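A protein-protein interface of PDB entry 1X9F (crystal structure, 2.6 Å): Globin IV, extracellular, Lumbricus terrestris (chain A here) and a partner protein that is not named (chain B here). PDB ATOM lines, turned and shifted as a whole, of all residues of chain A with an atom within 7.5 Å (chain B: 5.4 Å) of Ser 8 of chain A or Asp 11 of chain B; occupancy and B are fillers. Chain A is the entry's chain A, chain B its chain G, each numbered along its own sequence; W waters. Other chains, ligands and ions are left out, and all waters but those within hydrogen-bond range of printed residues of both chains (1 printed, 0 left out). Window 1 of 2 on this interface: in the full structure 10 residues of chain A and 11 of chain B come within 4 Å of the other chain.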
ATOM      1  N   ASP A   5       4.533 -12.359  25.209  1.00  0.00           N
ATOM      2  CA  ASP A   5       3.383 -12.076  26.120  1.00  0.00           C
ATOM      3  C   ASP A   5       2.503 -13.304  26.385  1.00  0.00           C
ATOM      4  O   ASP A   5       1.362 -13.183  26.839  1.00  0.00           O
ATOM      5  CB  ASP A   5       2.545 -10.907  25.589  1.00  0.00           C
ATOM      6  CG  ASP A   5       1.700 -11.287  24.381  1.00  0.00           C
ATOM      7  OD1 ASP A   5       2.093 -12.209  23.631  1.00  0.00           O
ATOM      8  OD2 ASP A   5       0.627 -10.712  24.098  1.00  0.00           O
ATOM      9  N   CYS A   6       3.037 -14.480  26.099  1.00  0.00           N
ATOM     10  CA  CYS A   6       2.361 -15.715  26.445  1.00  0.00           C
ATOM     11  C   CYS A   6       2.815 -16.051  27.855  1.00  0.00           C
ATOM     12  O   CYS A   6       3.875 -15.594  28.297  1.00  0.00           O
ATOM     13  CB  CYS A   6       2.766 -16.796  25.446  1.00  0.00           C
ATOM     14  SG  CYS A   6       2.903 -16.005  23.784  1.00  0.00           S
ATOM     15  N   CYS A   7       2.004 -16.823  28.566  1.00  0.00           N
ATOM     16  CA  CYS A   7       2.327 -17.262  29.914  1.00  0.00           C
ATOM     17  C   CYS A   7       3.120 -18.569  29.830  1.00  0.00           C
ATOM     18  O   CYS A   7       2.538 -19.645  29.666  1.00  0.00           O
ATOM     19  CB  CYS A   7       1.032 -17.436  30.712  1.00  0.00           C
ATOM     20  SG  CYS A   7       1.210 -18.116  32.376  1.00  0.00           S
ATOM     21  N   SER A   8       4.446 -18.470  29.929  1.00  0.00           N
ATOM     22  CA  SER A   8       5.317 -19.630  29.733  1.00  0.00           C
ATOM     23  C   SER A   8       5.219 -20.613  30.888  1.00  0.00           C
ATOM     24  O   SER A   8       4.589 -20.339  31.912  1.00  0.00           O
ATOM     25  CB  SER A   8       6.776 -19.198  29.540  1.00  0.00           C
ATOM     26  OG  SER A   8       7.447 -19.042  30.783  1.00  0.00           O
ATOM     27  N   TYR A   9       5.854 -21.761  30.711  1.00  0.00           N
ATOM     28  CA  TYR A   9       5.912 -22.752  31.759  1.00  0.00           C
ATOM     29  C   TYR A   9       6.766 -22.244  32.926  1.00  0.00           C
ATOM     30  O   TYR A   9       6.425 -22.457  34.092  1.00  0.00           O
ATOM     31  CB  TYR A   9       6.452 -24.072  31.213  1.00  0.00           C
ATOM     32  CG  TYR A   9       6.292 -25.184  32.200  1.00  0.00           C
ATOM     33  CD1 TYR A   9       5.144 -25.975  32.204  1.00  0.00           C
ATOM     34  CD2 TYR A   9       7.272 -25.423  33.165  1.00  0.00           C
ATOM     35  CE1 TYR A   9       4.982 -26.987  33.131  1.00  0.00           C
ATOM     36  CE2 TYR A   9       7.123 -26.424  34.097  1.00  0.00           C
ATOM     37  CZ  TYR A   9       5.976 -27.203  34.074  1.00  0.00           C
ATOM     38  OH  TYR A   9       5.824 -28.207  35.003  1.00  0.00           O
ATOM     39  N   GLU A  10       7.868 -21.572  32.602  1.00  0.00           N
ATOM     40  CA  GLU A  10       8.730 -20.944  33.603  1.00  0.00           C
ATOM     41  C   GLU A  10       7.971 -19.877  34.371  1.00  0.00           C
ATOM     42  O   GLU A  10       8.142 -19.734  35.586  1.00  0.00           O
ATOM     43  CB  GLU A  10       9.954 -20.304  32.944  1.00  0.00           C
ATOM     44  CG  GLU A  10      10.870 -21.282  32.221  1.00  0.00           C
ATOM     45  CD  GLU A  10      10.483 -21.517  30.765  1.00  0.00           C
ATOM     46  OE1 GLU A  10      11.392 -21.800  29.959  1.00  0.00           O
ATOM     47  OE2 GLU A  10       9.281 -21.427  30.418  1.00  0.00           O
ATOM     48  N   ASP A  11       7.143 -19.124  33.658  1.00  0.00           N
ATOM     49  CA  ASP A  11       6.375 -18.066  34.287  1.00  0.00           C
ATOM     50  C   ASP A  11       5.422 -18.653  35.308  1.00  0.00           C
ATOM     51  O   ASP A  11       5.260 -18.102  36.398  1.00  0.00           O
ATOM     52  CB  ASP A  11       5.571 -17.294  33.247  1.00  0.00           C
ATOM     53  CG  ASP A  11       6.437 -16.490  32.304  1.00  0.00           C
ATOM     54  OD1 ASP A  11       7.608 -16.182  32.638  1.00  0.00           O
ATOM     55  OD2 ASP A  11       6.007 -16.104  31.190  1.00  0.00           O
ATOM     56  N   ARG A  12       4.784 -19.764  34.947  1.00  0.00           N
ATOM     57  CA  ARG A  12       3.799 -20.398  35.818  1.00  0.00           C
ATOM     58  C   ARG A  12       4.475 -20.930  37.063  1.00  0.00           C
ATOM     59  O   ARG A  12       3.921 -20.872  38.162  1.00  0.00           O
ATOM     60  CB  ARG A  12       3.052 -21.505  35.079  1.00  0.00           C
ATOM     61  CG  ARG A  12       2.027 -20.952  34.106  1.00  0.00           C
ATOM     62  CD  ARG A  12       1.215 -22.006  33.398  1.00  0.00           C
ATOM     63  NE  ARG A  12       1.917 -22.541  32.235  1.00  0.00           N
ATOM     64  CZ  ARG A  12       1.922 -23.823  31.881  1.00  0.00           C
ATOM     65  NH1 ARG A  12       1.282 -24.732  32.612  1.00  0.00           N
ATOM     66  NH2 ARG A  12       2.587 -24.206  30.802  1.00  0.00           N
ATOM     67  N   ARG A  13       5.692 -21.420  36.888  1.00  0.00           N
ATOM     68  CA  ARG A  13       6.474 -21.926  37.991  1.00  0.00           C
ATOM     69  C   ARG A  13       6.939 -20.781  38.895  1.00  0.00           C
ATOM     70  O   ARG A  13       6.942 -20.908  40.122  1.00  0.00           O
ATOM     71  CB  ARG A  13       7.651 -22.714  37.431  1.00  0.00           C
ATOM     72  CG  ARG A  13       8.608 -23.245  38.477  1.00  0.00           C
ATOM     73  CD  ARG A  13       9.375 -24.429  37.959  1.00  0.00           C
ATOM     74  NE  ARG A  13      10.025 -24.116  36.694  1.00  0.00           N
ATOM     75  CZ  ARG A  13      10.626 -25.012  35.932  1.00  0.00           C
ATOM     76  NH1 ARG A  13      10.664 -26.296  36.294  1.00  0.00           N
ATOM     77  NH2 ARG A  13      11.194 -24.628  34.801  1.00  0.00           N
ATOM     78  N   GLU A  14       7.325 -19.670  38.275  1.00  0.00           N
ATOM     79  CA  GLU A  14       7.688 -18.462  38.997  1.00  0.00           C
ATOM     80  C   GLU A  14       6.540 -17.969  39.854  1.00  0.00           C
ATOM     81  O   GLU A  14       6.735 -17.585  41.010  1.00  0.00           O
ATOM     82  CB  GLU A  14       8.067 -17.362  38.009  1.00  0.00           C
ATOM     83  CG  GLU A  14       9.560 -17.174  37.842  1.00  0.00           C
ATOM     84  CD  GLU A  14      10.136 -16.174  38.826  1.00  0.00           C
ATOM     85  OE1 GLU A  14      11.168 -15.557  38.492  1.00  0.00           O
ATOM     86  OE2 GLU A  14       9.568 -15.993  39.928  1.00  0.00           O
ATOM     87  N   ILE A  15       5.343 -17.973  39.273  1.00  0.00           N
ATOM     88  CA  ILE A  15       4.155 -17.522  39.975  1.00  0.00           C
ATOM     89  C   ILE A  15       3.830 -18.416  41.167  1.00  0.00           C
ATOM     90  O   ILE A  15       3.313 -17.929  42.171  1.00  0.00           O
ATOM     91  CB  ILE A  15       2.970 -17.408  39.005  1.00  0.00           C
ATOM     92  CG1 ILE A  15       3.181 -16.183  38.119  1.00  0.00           C
ATOM     93  CG2 ILE A  15       1.649 -17.263  39.764  1.00  0.00           C
ATOM     94  CD1 ILE A  15       2.228 -16.088  36.989  1.00  0.00           C
ATOM     95  N   LEU A  84      -2.662 -23.657  37.538  1.00  0.00           N
ATOM     96  CA  LEU A  84      -1.645 -23.342  36.517  1.00  0.00           C
ATOM     97  C   LEU A  84      -0.867 -24.556  36.019  1.00  0.00           C
ATOM     98  O   LEU A  84      -0.163 -24.486  35.011  1.00  0.00           O
ATOM     99  CB  LEU A  84      -0.669 -22.271  37.013  1.00  0.00           C
ATOM    100  CG  LEU A  84      -1.233 -20.851  37.078  1.00  0.00           C
ATOM    101  CD1 LEU A  84      -0.221 -19.896  37.692  1.00  0.00           C
ATOM    102  CD2 LEU A  84      -1.686 -20.357  35.695  1.00  0.00           C
ATOM    103  N   ALA A 134       6.551 -11.642  34.888  1.00  0.00           N
ATOM    104  CA  ALA A 134       5.999 -12.989  34.827  1.00  0.00           C
ATOM    105  C   ALA A 134       4.563 -12.988  35.325  1.00  0.00           C
ATOM    106  O   ALA A 134       3.696 -13.618  34.710  1.00  0.00           O
ATOM    107  CB  ALA A 134       6.846 -13.962  35.633  1.00  0.00           C
ATOM    108  N   ARG A 137       2.176 -11.349  32.588  1.00  0.00           N
ATOM    109  CA  ARG A 137       1.990 -12.212  31.432  1.00  0.00           C
ATOM    110  C   ARG A 137       0.879 -13.218  31.664  1.00  0.00           C
ATOM    111  O   ARG A 137      -0.035 -13.359  30.848  1.00  0.00           O
ATOM    112  CB  ARG A 137       3.297 -12.936  31.109  1.00  0.00           C
ATOM    113  CG  ARG A 137       3.884 -12.532  29.774  1.00  0.00           C
ATOM    114  CD  ARG A 137       5.357 -12.181  29.801  1.00  0.00           C
ATOM    115  NE  ARG A 137       6.148 -13.086  30.629  1.00  0.00           N
ATOM    116  CZ  ARG A 137       7.316 -12.763  31.163  1.00  0.00           C
ATOM    117  NH1 ARG A 137       7.829 -11.554  30.961  1.00  0.00           N
ATOM    118  NH2 ARG A 137       7.977 -13.638  31.907  1.00  0.00           N
ATOM    119  N   CYS A 138       0.965 -13.889  32.805  1.00  0.00           N
ATOM    120  CA  CYS A 138       0.032 -14.928  33.172  1.00  0.00           C
ATOM    121  C   CYS A 138      -1.296 -14.372  33.615  1.00  0.00           C
ATOM    122  O   CYS A 138      -2.340 -14.910  33.250  1.00  0.00           O
ATOM    123  CB  CYS A 138       0.632 -15.788  34.267  1.00  0.00           C
ATOM    124  SG  CYS A 138       2.007 -16.765  33.656  1.00  0.00           S
ATOM    125  N   HIS B   5       8.607 -15.852  25.754  1.00  0.00           N
ATOM    126  CA  HIS B   5       7.753 -16.520  26.713  1.00  0.00           C
ATOM    127  C   HIS B   5       6.672 -17.305  25.994  1.00  0.00           C
ATOM    128  O   HIS B   5       5.789 -17.905  26.612  1.00  0.00           O
ATOM    129  CB  HIS B   5       7.162 -15.458  27.617  1.00  0.00           C
ATOM    130  CG  HIS B   5       8.186 -14.498  28.126  1.00  0.00           C
ATOM    131  ND1 HIS B   5       9.173 -14.877  29.009  1.00  0.00           N
ATOM    132  CD2 HIS B   5       8.397 -13.187  27.861  1.00  0.00           C
ATOM    133  CE1 HIS B   5       9.939 -13.838  29.280  1.00  0.00           C
ATOM    134  NE2 HIS B   5       9.488 -12.799  28.600  1.00  0.00           N
ATOM    135  N   CYS B   6       6.779 -17.290  24.670  1.00  0.00           N
ATOM    136  CA  CYS B   6       5.935 -18.077  23.798  1.00  0.00           C
ATOM    137  C   CYS B   6       6.732 -19.259  23.300  1.00  0.00           C
ATOM    138  O   CYS B   6       7.779 -19.087  22.669  1.00  0.00           O
ATOM    139  CB  CYS B   6       5.489 -17.234  22.617  1.00  0.00           C
ATOM    140  SG  CYS B   6       3.703 -17.286  22.434  1.00  0.00           S
ATOM    141  N   CYS B   7       6.234 -20.458  23.585  1.00  0.00           N
ATOM    142  CA  CYS B   7       6.976 -21.674  23.303  1.00  0.00           C
ATOM    143  C   CYS B   7       8.411 -21.502  23.790  1.00  0.00           C
ATOM    144  O   CYS B   7       9.365 -21.528  23.008  1.00  0.00           O
ATOM    145  CB  CYS B   7       6.939 -22.005  21.812  1.00  0.00           C
ATOM    146  SG  CYS B   7       7.519 -23.674  21.462  1.00  0.00           S
ATOM    147  N   SER B   8       8.548 -21.304  25.095  1.00  0.00           N
ATOM    148  CA  SER B   8       9.841 -21.084  25.718  1.00  0.00           C
ATOM    149  C   SER B   8      10.665 -22.362  25.788  1.00  0.00           C
ATOM    150  O   SER B   8      10.264 -23.408  25.268  1.00  0.00           O
ATOM    151  CB  SER B   8       9.642 -20.514  27.118  1.00  0.00           C
ATOM    152  OG  SER B   8       8.809 -21.368  27.884  1.00  0.00           O
ATOM    153  N   GLU B   9      11.826 -22.260  26.427  1.00  0.00           N
ATOM    154  CA  GLU B   9      12.721 -23.393  26.601  1.00  0.00           C
ATOM    155  C   GLU B   9      11.970 -24.538  27.262  1.00  0.00           C
ATOM    156  O   GLU B   9      11.881 -25.631  26.701  1.00  0.00           O
ATOM    157  CB  GLU B   9      13.935 -22.997  27.450  1.00  0.00           C
ATOM    158  CG  GLU B   9      14.895 -22.014  26.789  1.00  0.00           C
ATOM    159  CD  GLU B   9      15.665 -22.616  25.622  1.00  0.00           C
ATOM    160  OE1 GLU B   9      16.034 -21.855  24.699  1.00  0.00           O
ATOM    161  OE2 GLU B   9      15.910 -23.849  25.619  1.00  0.00           O
ATOM    162  N   GLU B  10      11.420 -24.275  28.451  1.00  0.00           N
ATOM    163  CA  GLU B  10      10.663 -25.286  29.187  1.00  0.00           C
ATOM    164  C   GLU B  10       9.406 -25.725  28.441  1.00  0.00           C
ATOM    165  O   GLU B  10       9.097 -26.914  28.420  1.00  0.00           O
ATOM    166  CB  GLU B  10      10.307 -24.802  30.596  1.00  0.00           C
ATOM    167  CG  GLU B  10      11.464 -24.865  31.578  1.00  0.00           C
ATOM    168  CD  GLU B  10      11.625 -26.241  32.189  1.00  0.00           C
ATOM    169  OE1 GLU B  10      10.893 -26.563  33.151  1.00  0.00           O
ATOM    170  OE2 GLU B  10      12.496 -26.998  31.710  1.00  0.00           O
ATOM    171  N   ASP B  11       8.702 -24.771  27.827  1.00  0.00           N
ATOM    172  CA  ASP B  11       7.540 -25.060  26.978  1.00  0.00           C
ATOM    173  C   ASP B  11       7.827 -26.149  25.952  1.00  0.00           C
ATOM    174  O   ASP B  11       7.096 -27.143  25.872  1.00  0.00           O
ATOM    175  CB  ASP B  11       7.089 -23.810  26.216  1.00  0.00           C
ATOM    176  CG  ASP B  11       6.215 -22.880  27.042  1.00  0.00           C
ATOM    177  OD1 ASP B  11       6.015 -21.727  26.598  1.00  0.00           O
ATOM    178  OD2 ASP B  11       5.682 -23.197  28.126  1.00  0.00           O
ATOM    179  N   HIS B  12       8.880 -25.964  25.158  1.00  0.00           N
ATOM    180  CA  HIS B  12       9.159 -26.928  24.101  1.00  0.00           C
ATOM    181  C   HIS B  12       9.679 -28.255  24.652  1.00  0.00           C
ATOM    182  O   HIS B  12       9.448 -29.313  24.065  1.00  0.00           O
ATOM    183  CB  HIS B  12      10.027 -26.338  22.971  1.00  0.00           C
ATOM    184  CG  HIS B  12      11.490 -26.233  23.282  1.00  0.00           C
ATOM    185  ND1 HIS B  12      12.170 -25.033  23.248  1.00  0.00           N
ATOM    186  CD2 HIS B  12      12.413 -27.179  23.581  1.00  0.00           C
ATOM    187  CE1 HIS B  12      13.442 -25.241  23.535  1.00  0.00           C
ATOM    188  NE2 HIS B  12      13.616 -26.533  23.744  1.00  0.00           N
ATOM    189  N   ARG B  13      10.352 -28.189  25.796  1.00  0.00           N
ATOM    190  CA  ARG B  13      10.797 -29.382  26.495  1.00  0.00           C
ATOM    191  C   ARG B  13       9.601 -30.216  26.977  1.00  0.00           C
ATOM    192  O   ARG B  13       9.638 -31.448  26.905  1.00  0.00           O
ATOM    193  CB  ARG B  13      11.705 -28.997  27.663  1.00  0.00           C
ATOM    194  CG  ARG B  13      12.497 -30.158  28.245  1.00  0.00           C
ATOM    195  CD  ARG B  13      13.208 -29.854  29.568  1.00  0.00           C
ATOM    196  NE  ARG B  13      12.317 -29.314  30.603  1.00  0.00           N
ATOM    197  CZ  ARG B  13      11.471 -30.035  31.343  1.00  0.00           C
ATOM    198  NH1 ARG B  13      11.375 -31.352  31.179  1.00  0.00           N
ATOM    199  NH2 ARG B  13      10.713 -29.434  32.252  1.00  0.00           N
ATOM    200  N   ILE B  14       8.552 -29.550  27.464  1.00  0.00           N
ATOM    201  CA  ILE B  14       7.329 -30.243  27.893  1.00  0.00           C
ATOM    202  C   ILE B  14       6.680 -30.938  26.697  1.00  0.00           C
ATOM    203  O   ILE B  14       6.345 -32.121  26.768  1.00  0.00           O
ATOM    204  CB  ILE B  14       6.326 -29.262  28.564  1.00  0.00           C
ATOM    205  CG1 ILE B  14       6.927 -28.603  29.814  1.00  0.00           C
ATOM    206  CG2 ILE B  14       5.003 -29.962  28.893  1.00  0.00           C
ATOM    207  CD1 ILE B  14       7.338 -29.565  30.928  1.00  0.00           C
ATOM    208  N   VAL B  15       6.523 -30.189  25.605  1.00  0.00           N
ATOM    209  CA  VAL B  15       5.920 -30.686  24.369  1.00  0.00           C
ATOM    210  C   VAL B  15       6.656 -31.933  23.866  1.00  0.00           C
ATOM    211  O   VAL B  15       6.021 -32.958  23.605  1.00  0.00           O
ATOM    212  CB  VAL B  15       5.856 -29.576  23.277  1.00  0.00           C
ATOM    213  CG1 VAL B  15       5.493 -30.152  21.912  1.00  0.00           C
ATOM    214  CG2 VAL B  15       4.865 -28.480  23.676  1.00  0.00           C
ATOM    215  N   GLN B  16       7.984 -31.851  23.759  1.00  0.00           N
ATOM    216  CA  GLN B  16       8.792 -32.984  23.284  1.00  0.00           C
ATOM    217  C   GLN B  16       8.646 -34.224  24.150  1.00  0.00           C
ATOM    218  O   GLN B  16       8.478 -35.324  23.620  1.00  0.00           O
ATOM    219  CB  GLN B  16      10.271 -32.603  23.167  1.00  0.00           C
ATOM    220  CG  GLN B  16      10.540 -31.625  22.030  1.00  0.00           C
ATOM    221  CD  GLN B  16      11.974 -31.143  22.025  1.00  0.00           C
ATOM    222  OE1 GLN B  16      12.557 -30.883  23.080  1.00  0.00           O
ATOM    223  NE2 GLN B  16      12.548 -31.017  20.834  1.00  0.00           N
ATOM    224  N   LEU B 134      -1.262 -25.308  27.637  1.00  0.00           N
ATOM    225  CA  LEU B 134      -0.652 -23.999  27.428  1.00  0.00           C
ATOM    226  C   LEU B 134       0.620 -24.068  26.593  1.00  0.00           C
ATOM    227  O   LEU B 134       0.773 -23.317  25.625  1.00  0.00           O
ATOM    228  CB  LEU B 134      -0.400 -23.298  28.763  1.00  0.00           C
ATOM    229  CG  LEU B 134      -1.659 -22.683  29.371  1.00  0.00           C
ATOM    230  CD1 LEU B 134      -1.399 -22.149  30.764  1.00  0.00           C
ATOM    231  CD2 LEU B 134      -2.236 -21.599  28.462  1.00  0.00           C
ATOM    232  N   ALA B 135       1.515 -24.978  26.966  1.00  0.00           N
ATOM    233  CA  ALA B 135       2.763 -25.188  26.243  1.00  0.00           C
ATOM    234  C   ALA B 135       2.500 -25.624  24.807  1.00  0.00           C
ATOM    235  O   ALA B 135       3.075 -25.061  23.873  1.00  0.00           O
ATOM    236  CB  ALA B 135       3.625 -26.211  26.966  1.00  0.00           C
ATOM    237  N   SER B 138       1.082 -22.682  22.491  1.00  0.00           N
ATOM    238  CA  SER B 138       2.059 -21.704  22.028  1.00  0.00           C
ATOM    239  C   SER B 138       3.012 -22.329  21.016  1.00  0.00           C
ATOM    240  O   SER B 138       3.308 -21.718  19.986  1.00  0.00           O
ATOM    241  CB  SER B 138       2.831 -21.092  23.196  1.00  0.00           C
ATOM    242  OG  SER B 138       3.546 -22.083  23.911  1.00  0.00           O
ATOM    243  N   CYS B 139       3.480 -23.543  21.299  1.00  0.00           N
ATOM    244  CA  CYS B 139       4.361 -24.225  20.361  1.00  0.00           C
ATOM    245  C   CYS B 139       3.654 -24.523  19.036  1.00  0.00           C
ATOM    246  O   CYS B 139       4.191 -24.205  17.977  1.00  0.00           O
ATOM    247  CB  CYS B 139       4.996 -25.464  20.996  1.00  0.00           C
ATOM    248  SG  CYS B 139       6.217 -25.013  22.266  1.00  0.00           S
HETATM  249  O   HOH W   1       3.073 -22.397  28.678  1.00  0.00           O
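The side-chain sulfur of Cys 6 of chain B is disulfide-bonded to the side-chain sulfur of Cys 6 of chain A, 2.0 Å away. N of Tyr 9 of chain A is in hydrogen-bond range of OD2 of Asp 11 of chain B, at 3.0 Å. The side-chain carboxylate (OE2) of Glu 10 of chain A sits at hydrogen-bond distance from the side-chain hydroxyl (OG) of Ser 8 of chain B. OE1 of Glu 10 of chain A lies within hydrogen-bond range of N of Glu 10 of chain B, at 2.9 Å. NH2 of Arg 13 of chain A is in salt-bridge range of OE1 of Glu 10 of chain B (2.6 Å). The guanidinium group of Arg 137 of chain A lies within hydrogen-bond range of a ring nitrogen (NE2) of His 5 of chain B (3.1 Å). O of Cys 6 of chain A lies close to O of His 5 of chain B (3.4 Å).
Water W1 lies within hydrogen-bond range of OD2 of Asp 11 of chain B, NH2 of Arg 12 of chain A, O of Cys 7 of chain A and N of Ala 135 of chain B.
The side-chain carboxylate (OE2) of Glu 10 of chain A lies within hydrogen-bond range of the side-chain hydroxyl (OG) of Ser 8 of chain A. NH2 of Arg 137 of chain A is in salt-bridge range of OD1 of Asp 11 of chain A, at 2.7 Å. The backbone NH (N) of Cys 7 of chain B sits at hydrogen-bond distance from the side-chain carboxylate (OD1) of Asp 11 of chain B, at 3.3 Å. OD1 of Asp 11 of chain B sits at hydrogen-bond distance from N of Ser 8 of chain B, 3.0 Å away. O of Ser 8 of chain B is in hydrogen-bond range of ND1 of His 12 of chain B, at 3.2 Å. O of Leu 134 of chain B sits at hydrogen-bond distance from OG of Ser 138 of chain B.
Ser 8 of chain A touches just these residues of chain B: His 5 (3.3 Å), Ser 8 (3.4 Å) and Asp 11 (3.8 Å). Of the printed residues of chain B, Tyr 9 of chain A touches Glu 10 (3.8 Å), Asp 11 (3.0 Å) and Ile 14 (3.97 Å). Of the printed residues of chain A, Glu 10 of chain B touches Tyr 9 (3.8 Å), Glu 10 (2.9 Å) and Arg 13 (2.6 Å). Of the printed residues of chain B, Arg 13 of chain A touches Glu 10. Of the printed residues of chain B, Arg 12 of chain A touches Leu 134. Val 15 of chain B touches none of the printed residues of chain A. The nearest residue of chain B that does not touch Ser 8 of chain A is Cys 6 of chain B (5.2 Å). The nearest residue of chain A that does not touch Asp 11 of chain B is Arg 12 of chain A (4.2 Å). The nearest printed residue of chain B that does not touch Cys 6 of chain A is Ser 138 of chain B (4.8 Å).
Ser 8 of chain A touches His 5 of chain B (CB to O, 3.3 Å). Ser 8 of chain B touches Ser 8 of chain A. Ser 8 of chain A touches Asp 11 of chain B (C to OD2, 3.8 Å). Tyr 9 of chain A touches Glu 10 of chain B. Tyr 9 of chain A touches Ile 14 of chain B (CD1 to CG1, 3.97 Å). Glu 9 of chain B touches Glu 10 of chain A. Asp 11 of chain A touches His 5 of chain B (OD2 to CB, 3.8 Å). Arg 12 of chain A touches Leu 134 of chain B (NE to CD1, 3.6 Å).
Of the 16 printed residues of chain B, 8 touch a printed residue of chain A. Hydrophobic or aromatic side chains of chain B that line the printed part of chain A: His 5, Ile 14 and Leu 134. Of the 15 printed residues of chain A, 8 touch a printed residue of chain B. Printed residues of chain A that touch a printed residue of chain B: Cys 6, Ser 8, Tyr 9, Glu 10, Asp 11, Arg 12, Arg 13 and Arg 137. Among the printed residues, Asp or Glu carboxylates within 4 Å of a Lys or Arg side-chain nitrogen of the other chain: Arg 13 of chain A with Glu 10 of chain B (2.6 Å).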
